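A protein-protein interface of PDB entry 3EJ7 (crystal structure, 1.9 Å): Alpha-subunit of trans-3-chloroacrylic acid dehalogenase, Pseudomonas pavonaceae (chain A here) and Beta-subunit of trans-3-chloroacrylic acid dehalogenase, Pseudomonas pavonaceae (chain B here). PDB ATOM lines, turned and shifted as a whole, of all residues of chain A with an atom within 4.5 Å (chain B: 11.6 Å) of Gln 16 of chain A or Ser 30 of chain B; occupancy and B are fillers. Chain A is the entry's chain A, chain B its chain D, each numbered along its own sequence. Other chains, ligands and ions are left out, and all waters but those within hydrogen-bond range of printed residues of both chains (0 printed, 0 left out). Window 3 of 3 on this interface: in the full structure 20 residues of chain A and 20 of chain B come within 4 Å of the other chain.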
ATOM      1  N   ARG A  12      34.595  12.278 -13.833  1.00  0.00           N
ATOM      2  CA  ARG A  12      34.568  13.735 -13.647  1.00  0.00           C
ATOM      3  C   ARG A  12      35.981  14.280 -13.488  1.00  0.00           C
ATOM      4  O   ARG A  12      36.828  13.631 -12.889  1.00  0.00           O
ATOM      5  CB  ARG A  12      33.695  14.158 -12.460  1.00  0.00           C
ATOM      6  CG  ARG A  12      32.367  14.842 -12.851  1.00  0.00           C
ATOM      7  CD  ARG A  12      31.388  13.940 -13.609  1.00  0.00           C
ATOM      8  NE  ARG A  12      30.722  13.035 -12.681  1.00  0.00           N
ATOM      9  CZ  ARG A  12      30.446  11.752 -12.910  1.00  0.00           C
ATOM     10  NH1 ARG A  12      29.847  11.058 -11.971  1.00  0.00           N
ATOM     11  NH2 ARG A  12      30.777  11.163 -14.066  1.00  0.00           N
ATOM     12  N   THR A  13      36.214  15.467 -14.058  1.00  0.00           N
ATOM     13  CA  THR A  13      37.501  16.168 -13.962  1.00  0.00           C
ATOM     14  C   THR A  13      37.783  16.719 -12.551  1.00  0.00           C
ATOM     15  O   THR A  13      36.864  16.841 -11.727  1.00  0.00           O
ATOM     16  CB  THR A  13      37.565  17.330 -14.955  1.00  0.00           C
ATOM     17  OG1 THR A  13      36.488  18.241 -14.693  1.00  0.00           O
ATOM     18  CG2 THR A  13      37.476  16.825 -16.405  1.00  0.00           C
ATOM     19  N   ASP A  14      39.051  17.022 -12.254  1.00  0.00           N
ATOM     20  CA  ASP A  14      39.387  17.636 -10.959  1.00  0.00           C
ATOM     21  C   ASP A  14      38.636  18.972 -10.840  1.00  0.00           C
ATOM     22  O   ASP A  14      38.135  19.294  -9.769  1.00  0.00           O
ATOM     23  CB  ASP A  14      40.910  17.862 -10.781  1.00  0.00           C
ATOM     24  CG  ASP A  14      41.705  16.557 -10.551  1.00  0.00           C
ATOM     25  OD1 ASP A  14      42.948  16.644 -10.380  1.00  0.00           O
ATOM     26  OD2 ASP A  14      41.121  15.446 -10.569  1.00  0.00           O
ATOM     27  N   GLU A  15      38.521  19.726 -11.938  1.00  0.00           N
ATOM     28  CA  GLU A  15      37.762  20.982 -11.887  1.00  0.00           C
ATOM     29  C   GLU A  15      36.297  20.785 -11.517  1.00  0.00           C
ATOM     30  O   GLU A  15      35.741  21.555 -10.746  1.00  0.00           O
ATOM     31  CB  GLU A  15      37.881  21.803 -13.167  1.00  0.00           C
ATOM     32  CG  GLU A  15      39.095  22.733 -13.188  1.00  0.00           C
ATOM     33  CD  GLU A  15      39.071  23.794 -12.075  1.00  0.00           C
ATOM     34  OE1 GLU A  15      38.198  24.698 -12.145  1.00  0.00           O
ATOM     35  OE2 GLU A  15      39.934  23.742 -11.150  1.00  0.00           O
ATOM     36  N   GLN A  16      35.676  19.751 -12.072  1.00  0.00           N
ATOM     37  CA  GLN A  16      34.276  19.475 -11.754  1.00  0.00           C
ATOM     38  C   GLN A  16      34.131  19.087 -10.303  1.00  0.00           C
ATOM     39  O   GLN A  16      33.130  19.434  -9.668  1.00  0.00           O
ATOM     40  CB  GLN A  16      33.720  18.384 -12.650  1.00  0.00           C
ATOM     41  CG  GLN A  16      33.491  18.816 -14.116  1.00  0.00           C
ATOM     42  CD  GLN A  16      32.922  17.680 -14.922  1.00  0.00           C
ATOM     43  OE1 GLN A  16      33.503  16.578 -14.978  1.00  0.00           O
ATOM     44  NE2 GLN A  16      31.757  17.915 -15.529  1.00  0.00           N
ATOM     45  N   LYS A  17      35.124  18.368  -9.775  1.00  0.00           N
ATOM     46  CA  LYS A  17      35.073  17.933  -8.394  1.00  0.00           C
ATOM     47  C   LYS A  17      35.194  19.121  -7.449  1.00  0.00           C
ATOM     48  O   LYS A  17      34.543  19.158  -6.393  1.00  0.00           O
ATOM     49  CB  LYS A  17      36.107  16.814  -8.093  1.00  0.00           C
ATOM     50  CG  LYS A  17      35.889  15.515  -8.899  1.00  0.00           C
ATOM     51  CD  LYS A  17      36.869  14.425  -8.481  1.00  0.00           C
ATOM     52  CE  LYS A  17      36.664  13.157  -9.259  1.00  0.00           C
ATOM     53  NZ  LYS A  17      37.798  12.208  -8.977  1.00  0.00           N
ATOM     54  N   ARG A  18      36.014  20.092  -7.832  1.00  0.00           N
ATOM     55  CA  ARG A  18      36.182  21.317  -7.051  1.00  0.00           C
ATOM     56  C   ARG A  18      34.912  22.163  -7.036  1.00  0.00           C
ATOM     57  O   ARG A  18      34.604  22.815  -6.037  1.00  0.00           O
ATOM     58  CB  ARG A  18      37.342  22.147  -7.593  1.00  0.00           C
ATOM     59  CG  ARG A  18      38.664  21.415  -7.610  1.00  0.00           C
ATOM     60  CD  ARG A  18      39.827  22.388  -7.717  1.00  0.00           C
ATOM     61  NE  ARG A  18      40.338  22.743  -6.395  1.00  0.00           N
ATOM     62  CZ  ARG A  18      41.469  22.276  -5.873  1.00  0.00           C
ATOM     63  NH1 ARG A  18      42.238  21.436  -6.560  1.00  0.00           N
ATOM     64  NH2 ARG A  18      41.844  22.659  -4.660  1.00  0.00           N
ATOM     65  N   ALA A  19      34.187  22.164  -8.155  1.00  0.00           N
ATOM     66  CA  ALA A  19      32.904  22.865  -8.260  1.00  0.00           C
ATOM     67  C   ALA A  19      31.885  22.179  -7.345  1.00  0.00           C
ATOM     68  O   ALA A  19      31.178  22.836  -6.574  1.00  0.00           O
ATOM     69  CB  ALA A  19      32.419  22.844  -9.690  1.00  0.00           C
ATOM     70  N   LEU A  20      31.832  20.853  -7.441  1.00  0.00           N
ATOM     71  CA  LEU A  20      30.962  20.020  -6.608  1.00  0.00           C
ATOM     72  C   LEU A  20      31.142  20.297  -5.110  1.00  0.00           C
ATOM     73  O   LEU A  20      30.166  20.550  -4.379  1.00  0.00           O
ATOM     74  CB  LEU A  20      31.211  18.537  -6.924  1.00  0.00           C
ATOM     75  CG  LEU A  20      30.358  17.561  -6.127  1.00  0.00           C
ATOM     76  CD1 LEU A  20      28.871  17.805  -6.461  1.00  0.00           C
ATOM     77  CD2 LEU A  20      30.778  16.092  -6.336  1.00  0.00           C
ATOM     78  N   PRO B   1      24.421   9.813  -8.915  1.00  0.00           N
ATOM     79  CA  PRO B   1      25.259   9.823  -7.727  1.00  0.00           C
ATOM     80  C   PRO B   1      24.440   9.553  -6.448  1.00  0.00           C
ATOM     81  O   PRO B   1      23.192   9.595  -6.483  1.00  0.00           O
ATOM     82  CB  PRO B   1      25.794  11.255  -7.691  1.00  0.00           C
ATOM     83  CG  PRO B   1      25.794  11.704  -9.104  1.00  0.00           C
ATOM     84  CD  PRO B   1      24.674  10.974  -9.796  1.00  0.00           C
ATOM     85  N   ILE B   3      24.547  11.103  -2.587  1.00  0.00           N
ATOM     86  CA  ILE B   3      25.156  12.052  -1.645  1.00  0.00           C
ATOM     87  C   ILE B   3      24.538  11.746  -0.265  1.00  0.00           C
ATOM     88  O   ILE B   3      23.298  11.798  -0.073  1.00  0.00           O
ATOM     89  CB  ILE B   3      24.949  13.548  -2.020  1.00  0.00           C
ATOM     90  CG1 ILE B   3      25.482  13.897  -3.419  1.00  0.00           C
ATOM     91  CG2 ILE B   3      25.644  14.481  -0.991  1.00  0.00           C
ATOM     92  CD1 ILE B   3      24.442  13.759  -4.513  1.00  0.00           C
ATOM     93  N   ARG B  21      17.008  20.126  -1.655  1.00  0.00           N
ATOM     94  CA  ARG B  21      16.808  20.810  -2.934  1.00  0.00           C
ATOM     95  C   ARG B  21      18.112  21.447  -3.433  1.00  0.00           C
ATOM     96  O   ARG B  21      18.459  21.353  -4.628  1.00  0.00           O
ATOM     97  CB  ARG B  21      15.733  21.892  -2.757  1.00  0.00           C
ATOM     98  CG  ARG B  21      14.860  22.103  -3.955  1.00  0.00           C
ATOM     99  CD  ARG B  21      13.763  23.137  -3.669  1.00  0.00           C
ATOM    100  NE  ARG B  21      12.817  22.710  -2.633  1.00  0.00           N
ATOM    101  CZ  ARG B  21      11.792  21.886  -2.835  1.00  0.00           C
ATOM    102  NH1 ARG B  21      10.983  21.583  -1.838  1.00  0.00           N
ATOM    103  NH2 ARG B  21      11.575  21.357  -4.031  1.00  0.00           N
ATOM    104  N   ASP B  22      18.806  22.127  -2.518  1.00  0.00           N
ATOM    105  CA  ASP B  22      20.090  22.785  -2.808  1.00  0.00           C
ATOM    106  C   ASP B  22      21.228  21.771  -3.176  1.00  0.00           C
ATOM    107  O   ASP B  22      21.999  22.042  -4.118  1.00  0.00           O
ATOM    108  CB  ASP B  22      20.507  23.715  -1.652  1.00  0.00           C
ATOM    109  CG  ASP B  22      19.620  24.969  -1.522  1.00  0.00           C
ATOM    110  OD1 ASP B  22      19.900  25.796  -0.625  1.00  0.00           O
ATOM    111  OD2 ASP B  22      18.641  25.146  -2.287  1.00  0.00           O
ATOM    112  N   VAL B  23      21.313  20.639  -2.462  1.00  0.00           N
ATOM    113  CA  VAL B  23      22.258  19.529  -2.778  1.00  0.00           C
ATOM    114  C   VAL B  23      22.033  18.998  -4.197  1.00  0.00           C
ATOM    115  O   VAL B  23      22.985  18.797  -4.937  1.00  0.00           O
ATOM    116  CB  VAL B  23      22.227  18.325  -1.749  1.00  0.00           C
ATOM    117  CG1 VAL B  23      22.954  17.068  -2.314  1.00  0.00           C
ATOM    118  CG2 VAL B  23      22.832  18.721  -0.411  1.00  0.00           C
ATOM    119  N   ILE B  24      20.775  18.766  -4.558  1.00  0.00           N
ATOM    120  CA  ILE B  24      20.431  18.283  -5.907  1.00  0.00           C
ATOM    121  C   ILE B  24      20.868  19.279  -6.968  1.00  0.00           C
ATOM    122  O   ILE B  24      21.572  18.882  -7.907  1.00  0.00           O
ATOM    123  CB  ILE B  24      18.927  17.913  -6.063  1.00  0.00           C
ATOM    124  CG1 ILE B  24      18.578  16.712  -5.185  1.00  0.00           C
ATOM    125  CG2 ILE B  24      18.609  17.601  -7.532  1.00  0.00           C
ATOM    126  CD1 ILE B  24      17.064  16.608  -4.842  1.00  0.00           C
ATOM    127  N   ASP B  25      20.495  20.556  -6.792  1.00  0.00           N
ATOM    128  CA  ASP B  25      20.853  21.618  -7.739  1.00  0.00           C
ATOM    129  C   ASP B  25      22.358  21.729  -7.941  1.00  0.00           C
ATOM    130  O   ASP B  25      22.824  21.766  -9.085  1.00  0.00           O
ATOM    131  CB  ASP B  25      20.326  23.000  -7.332  1.00  0.00           C
ATOM    132  CG  ASP B  25      20.607  24.075  -8.403  1.00  0.00           C
ATOM    133  OD1 ASP B  25      21.373  25.048  -8.139  1.00  0.00           O
ATOM    134  OD2 ASP B  25      20.072  23.954  -9.539  1.00  0.00           O
ATOM    135  N   VAL B  26      23.094  21.813  -6.832  1.00  0.00           N
ATOM    136  CA  VAL B  26      24.555  21.870  -6.866  1.00  0.00           C
ATOM    137  C   VAL B  26      25.189  20.689  -7.608  1.00  0.00           C
ATOM    138  O   VAL B  26      26.143  20.868  -8.369  1.00  0.00           O
ATOM    139  CB  VAL B  26      25.171  22.008  -5.459  1.00  0.00           C
ATOM    140  CG1 VAL B  26      26.674  21.630  -5.489  1.00  0.00           C
ATOM    141  CG2 VAL B  26      24.994  23.437  -4.970  1.00  0.00           C
ATOM    142  N   THR B  27      24.645  19.500  -7.404  1.00  0.00           N
ATOM    143  CA  THR B  27      25.214  18.297  -7.993  1.00  0.00           C
ATOM    144  C   THR B  27      24.998  18.340  -9.487  1.00  0.00           C
ATOM    145  O   THR B  27      25.924  18.106 -10.253  1.00  0.00           O
ATOM    146  CB  THR B  27      24.622  17.021  -7.340  1.00  0.00           C
ATOM    147  OG1 THR B  27      24.937  17.031  -5.939  1.00  0.00           O
ATOM    148  CG2 THR B  27      25.183  15.736  -7.973  1.00  0.00           C
ATOM    149  N   ASN B  28      23.776  18.696  -9.892  1.00  0.00           N
ATOM    150  CA  ASN B  28      23.438  18.837 -11.294  1.00  0.00           C
ATOM    151  C   ASN B  28      24.289  19.903 -12.035  1.00  0.00           C
ATOM    152  O   ASN B  28      24.747  19.663 -13.151  1.00  0.00           O
ATOM    153  CB  ASN B  28      21.937  19.101 -11.431  1.00  0.00           C
ATOM    154  CG  ASN B  28      21.532  19.416 -12.835  1.00  0.00           C
ATOM    155  OD1 ASN B  28      21.201  20.561 -13.148  1.00  0.00           O
ATOM    156  ND2 ASN B  28      21.574  18.412 -13.711  1.00  0.00           N
ATOM    157  N   LYS B  29      24.492  21.063 -11.401  1.00  0.00           N
ATOM    158  CA  LYS B  29      25.252  22.173 -11.985  1.00  0.00           C
ATOM    159  C   LYS B  29      26.745  21.892 -12.148  1.00  0.00           C
ATOM    160  O   LYS B  29      27.375  22.344 -13.097  1.00  0.00           O
ATOM    161  CB  LYS B  29      25.092  23.409 -11.106  1.00  0.00           C
ATOM    162  CG  LYS B  29      24.089  24.426 -11.635  1.00  0.00           C
ATOM    163  CD  LYS B  29      22.672  23.856 -11.752  1.00  0.00           C
ATOM    164  CE  LYS B  29      21.993  24.412 -13.005  1.00  0.00           C
ATOM    165  NZ  LYS B  29      21.892  25.890 -12.915  1.00  0.00           N
ATOM    166  N   SER B  30      27.314  21.176 -11.196  1.00  0.00           N
ATOM    167  CA  SER B  30      28.759  21.053 -11.095  1.00  0.00           C
ATOM    168  C   SER B  30      29.318  19.845 -11.868  1.00  0.00           C
ATOM    169  O   SER B  30      30.376  19.940 -12.488  1.00  0.00           O
ATOM    170  CB  SER B  30      29.131  20.956  -9.615  1.00  0.00           C
ATOM    171  OG  SER B  30      28.526  19.813  -9.037  1.00  0.00           O
ATOM    172  N   ILE B  31      28.606  18.717 -11.813  1.00  0.00           N
ATOM    173  CA  ILE B  31      29.088  17.481 -12.445  1.00  0.00           C
ATOM    174  C   ILE B  31      28.176  16.984 -13.580  1.00  0.00           C
ATOM    175  O   ILE B  31      28.495  16.004 -14.256  1.00  0.00           O
ATOM    176  CB  ILE B  31      29.414  16.374 -11.396  1.00  0.00           C
ATOM    177  CG1 ILE B  31      28.119  15.769 -10.801  1.00  0.00           C
ATOM    178  CG2 ILE B  31      30.393  16.927 -10.327  1.00  0.00           C
ATOM    179  CD1 ILE B  31      28.334  14.677  -9.733  1.00  0.00           C
ATOM    180  N   GLY B  32      27.050  17.679 -13.774  1.00  0.00           N
ATOM    181  CA  GLY B  32      26.184  17.493 -14.944  1.00  0.00           C
ATOM    182  C   GLY B  32      25.178  16.359 -14.853  1.00  0.00           C
ATOM    183  O   GLY B  32      24.522  16.032 -15.834  1.00  0.00           O
ATOM    184  N   SER B  33      25.045  15.764 -13.674  1.00  0.00           N
ATOM    185  CA  SER B  33      24.120  14.650 -13.456  1.00  0.00           C
ATOM    186  C   SER B  33      22.639  15.024 -13.629  1.00  0.00           C
ATOM    187  O   SER B  33      22.181  16.028 -13.069  1.00  0.00           O
ATOM    188  CB  SER B  33      24.342  14.081 -12.054  1.00  0.00           C
ATOM    189  OG  SER B  33      25.553  13.360 -12.004  1.00  0.00           O
ATOM    190  N   ASP B  34      21.895  14.221 -14.391  1.00  0.00           N
ATOM    191  CA  ASP B  34      20.438  14.397 -14.460  1.00  0.00           C
ATOM    192  C   ASP B  34      19.867  14.183 -13.052  1.00  0.00           C
ATOM    193  O   ASP B  34      20.208  13.185 -12.392  1.00  0.00           O
ATOM    194  CB  ASP B  34      19.788  13.419 -15.448  1.00  0.00           C
ATOM    195  CG  ASP B  34      18.343  13.813 -15.818  1.00  0.00           C
ATOM    196  OD1 ASP B  34      17.464  13.887 -14.934  1.00  0.00           O
ATOM    197  OD2 ASP B  34      18.076  14.045 -17.020  1.00  0.00           O
ATOM    198  N   PRO B  35      19.034  15.134 -12.569  1.00  0.00           N
ATOM    199  CA  PRO B  35      18.365  14.970 -11.280  1.00  0.00           C
ATOM    200  C   PRO B  35      17.728  13.594 -11.115  1.00  0.00           C
ATOM    201  O   PRO B  35      17.598  13.117  -9.995  1.00  0.00           O
ATOM    202  CB  PRO B  35      17.306  16.075 -11.276  1.00  0.00           C
ATOM    203  CG  PRO B  35      17.347  16.681 -12.658  1.00  0.00           C
ATOM    204  CD  PRO B  35      18.697  16.427 -13.183  1.00  0.00           C
ATOM    205  N   ILE B  37      19.083  10.753 -11.766  1.00  0.00           N
ATOM    206  CA  ILE B  37      20.058   9.811 -11.170  1.00  0.00           C
ATOM    207  C   ILE B  37      20.695  10.348  -9.876  1.00  0.00           C
ATOM    208  O   ILE B  37      21.605   9.712  -9.341  1.00  0.00           O
ATOM    209  CB  ILE B  37      21.164   9.335 -12.178  1.00  0.00           C
ATOM    210  CG1 ILE B  37      21.915  10.537 -12.761  1.00  0.00           C
ATOM    211  CG2 ILE B  37      20.572   8.467 -13.310  1.00  0.00           C
ATOM    212  CD1 ILE B  37      23.315  10.218 -13.243  1.00  0.00           C
ATOM    213  N   ILE B  38      20.220  11.494  -9.368  1.00  0.00           N
ATOM    214  CA  ILE B  38      20.756  12.095  -8.104  1.00  0.00           C
ATOM    215  C   ILE B  38      19.955  11.605  -6.890  1.00  0.00           C
ATOM    216  O   ILE B  38      18.719  11.774  -6.807  1.00  0.00           O
ATOM    217  CB  ILE B  38      20.822  13.667  -8.138  1.00  0.00           C
ATOM    218  CG1 ILE B  38      21.712  14.147  -9.286  1.00  0.00           C
ATOM    219  CG2 ILE B  38      21.325  14.220  -6.769  1.00  0.00           C
ATOM    220  CD1 ILE B  38      21.706  15.683  -9.534  1.00  0.00           C
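Among the printed residues, pairs that only touch across the chains: Leu 20 of chain A with Ser 30 of chain B (3.3 Å), Arg 12 of chain A with Ile 31 of chain B (3.6 Å), Gln 16 of chain A with Ser 30 of chain B (3.7 Å), Gln 16 of chain A with Ile 31 of chain B (3.8 Å), Ala 19 of chain A with Ser 30 of chain B (3.8 Å), Leu 20 of chain A with Val 26 of chain B (3.8 Å), Leu 20 of chain A with Ile 31 of chain B (3.9 Å) and Leu 20 of chain A with Thr 27 of chain B (3.995 Å).
The backbone NH of Thr 13 of chain A sits at hydrogen-bond distance from the side-chain amide oxygen of Gln 16 of chain A (3.1 Å).
O of Val 23 of chain B is in hydrogen-bond range of OG1 of Thr 27 of chain B (2.8 Å).
O of Val 26 of chain B is in hydrogen-bond range of OG of Ser 30 of chain B (2.7 Å).
The backbone carbonyl oxygen (O) of Thr 27 of chain B is in hydrogen-bond range of the side-chain hydroxyl (OG) of Ser 30 of chain B, 3.3 Å away.
Among the printed residues, 8 pairs touch across the chains.
Among the printed residues, no Asp or Glu carboxylate lies within 4 Å of a Lys or Arg side-chain nitrogen of the other chain.
Of chain B, only Ser 30 and Ile 31 come within 4 Å of Gln 16 of chain A.
Of chain A, only Gln 16 (3.7 Å), Ala 19 (3.8 Å) and Leu 20 (3.3 Å) come within 4 Å of Ser 30 of chain B.
No residue of chain B comes within 4 Å of Glu 15 of chain A.
Of the printed residues of chain A, Val 26 of chain B touches Leu 20 (3.8 Å).
Of the printed residues of chain A, Thr 27 of chain B touches Leu 20 (3.995 Å).
Printed residues of chain B within 4 Å of Arg 12 of chain A: Ile 31.
Arg 18 of chain A touches none of the printed residues of chain B.
The nearest residue of chain B that does not touch Gln 16 of chain A is Gly 32 of chain B (5.0 Å).
The nearest printed residue of chain A that does not touch Ser 30 of chain B is Arg 12 of chain A (5.5 Å).
The nearest printed residue of chain A that does not touch Ile 31 of chain B is Lys 17 of chain A (5.0 Å).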
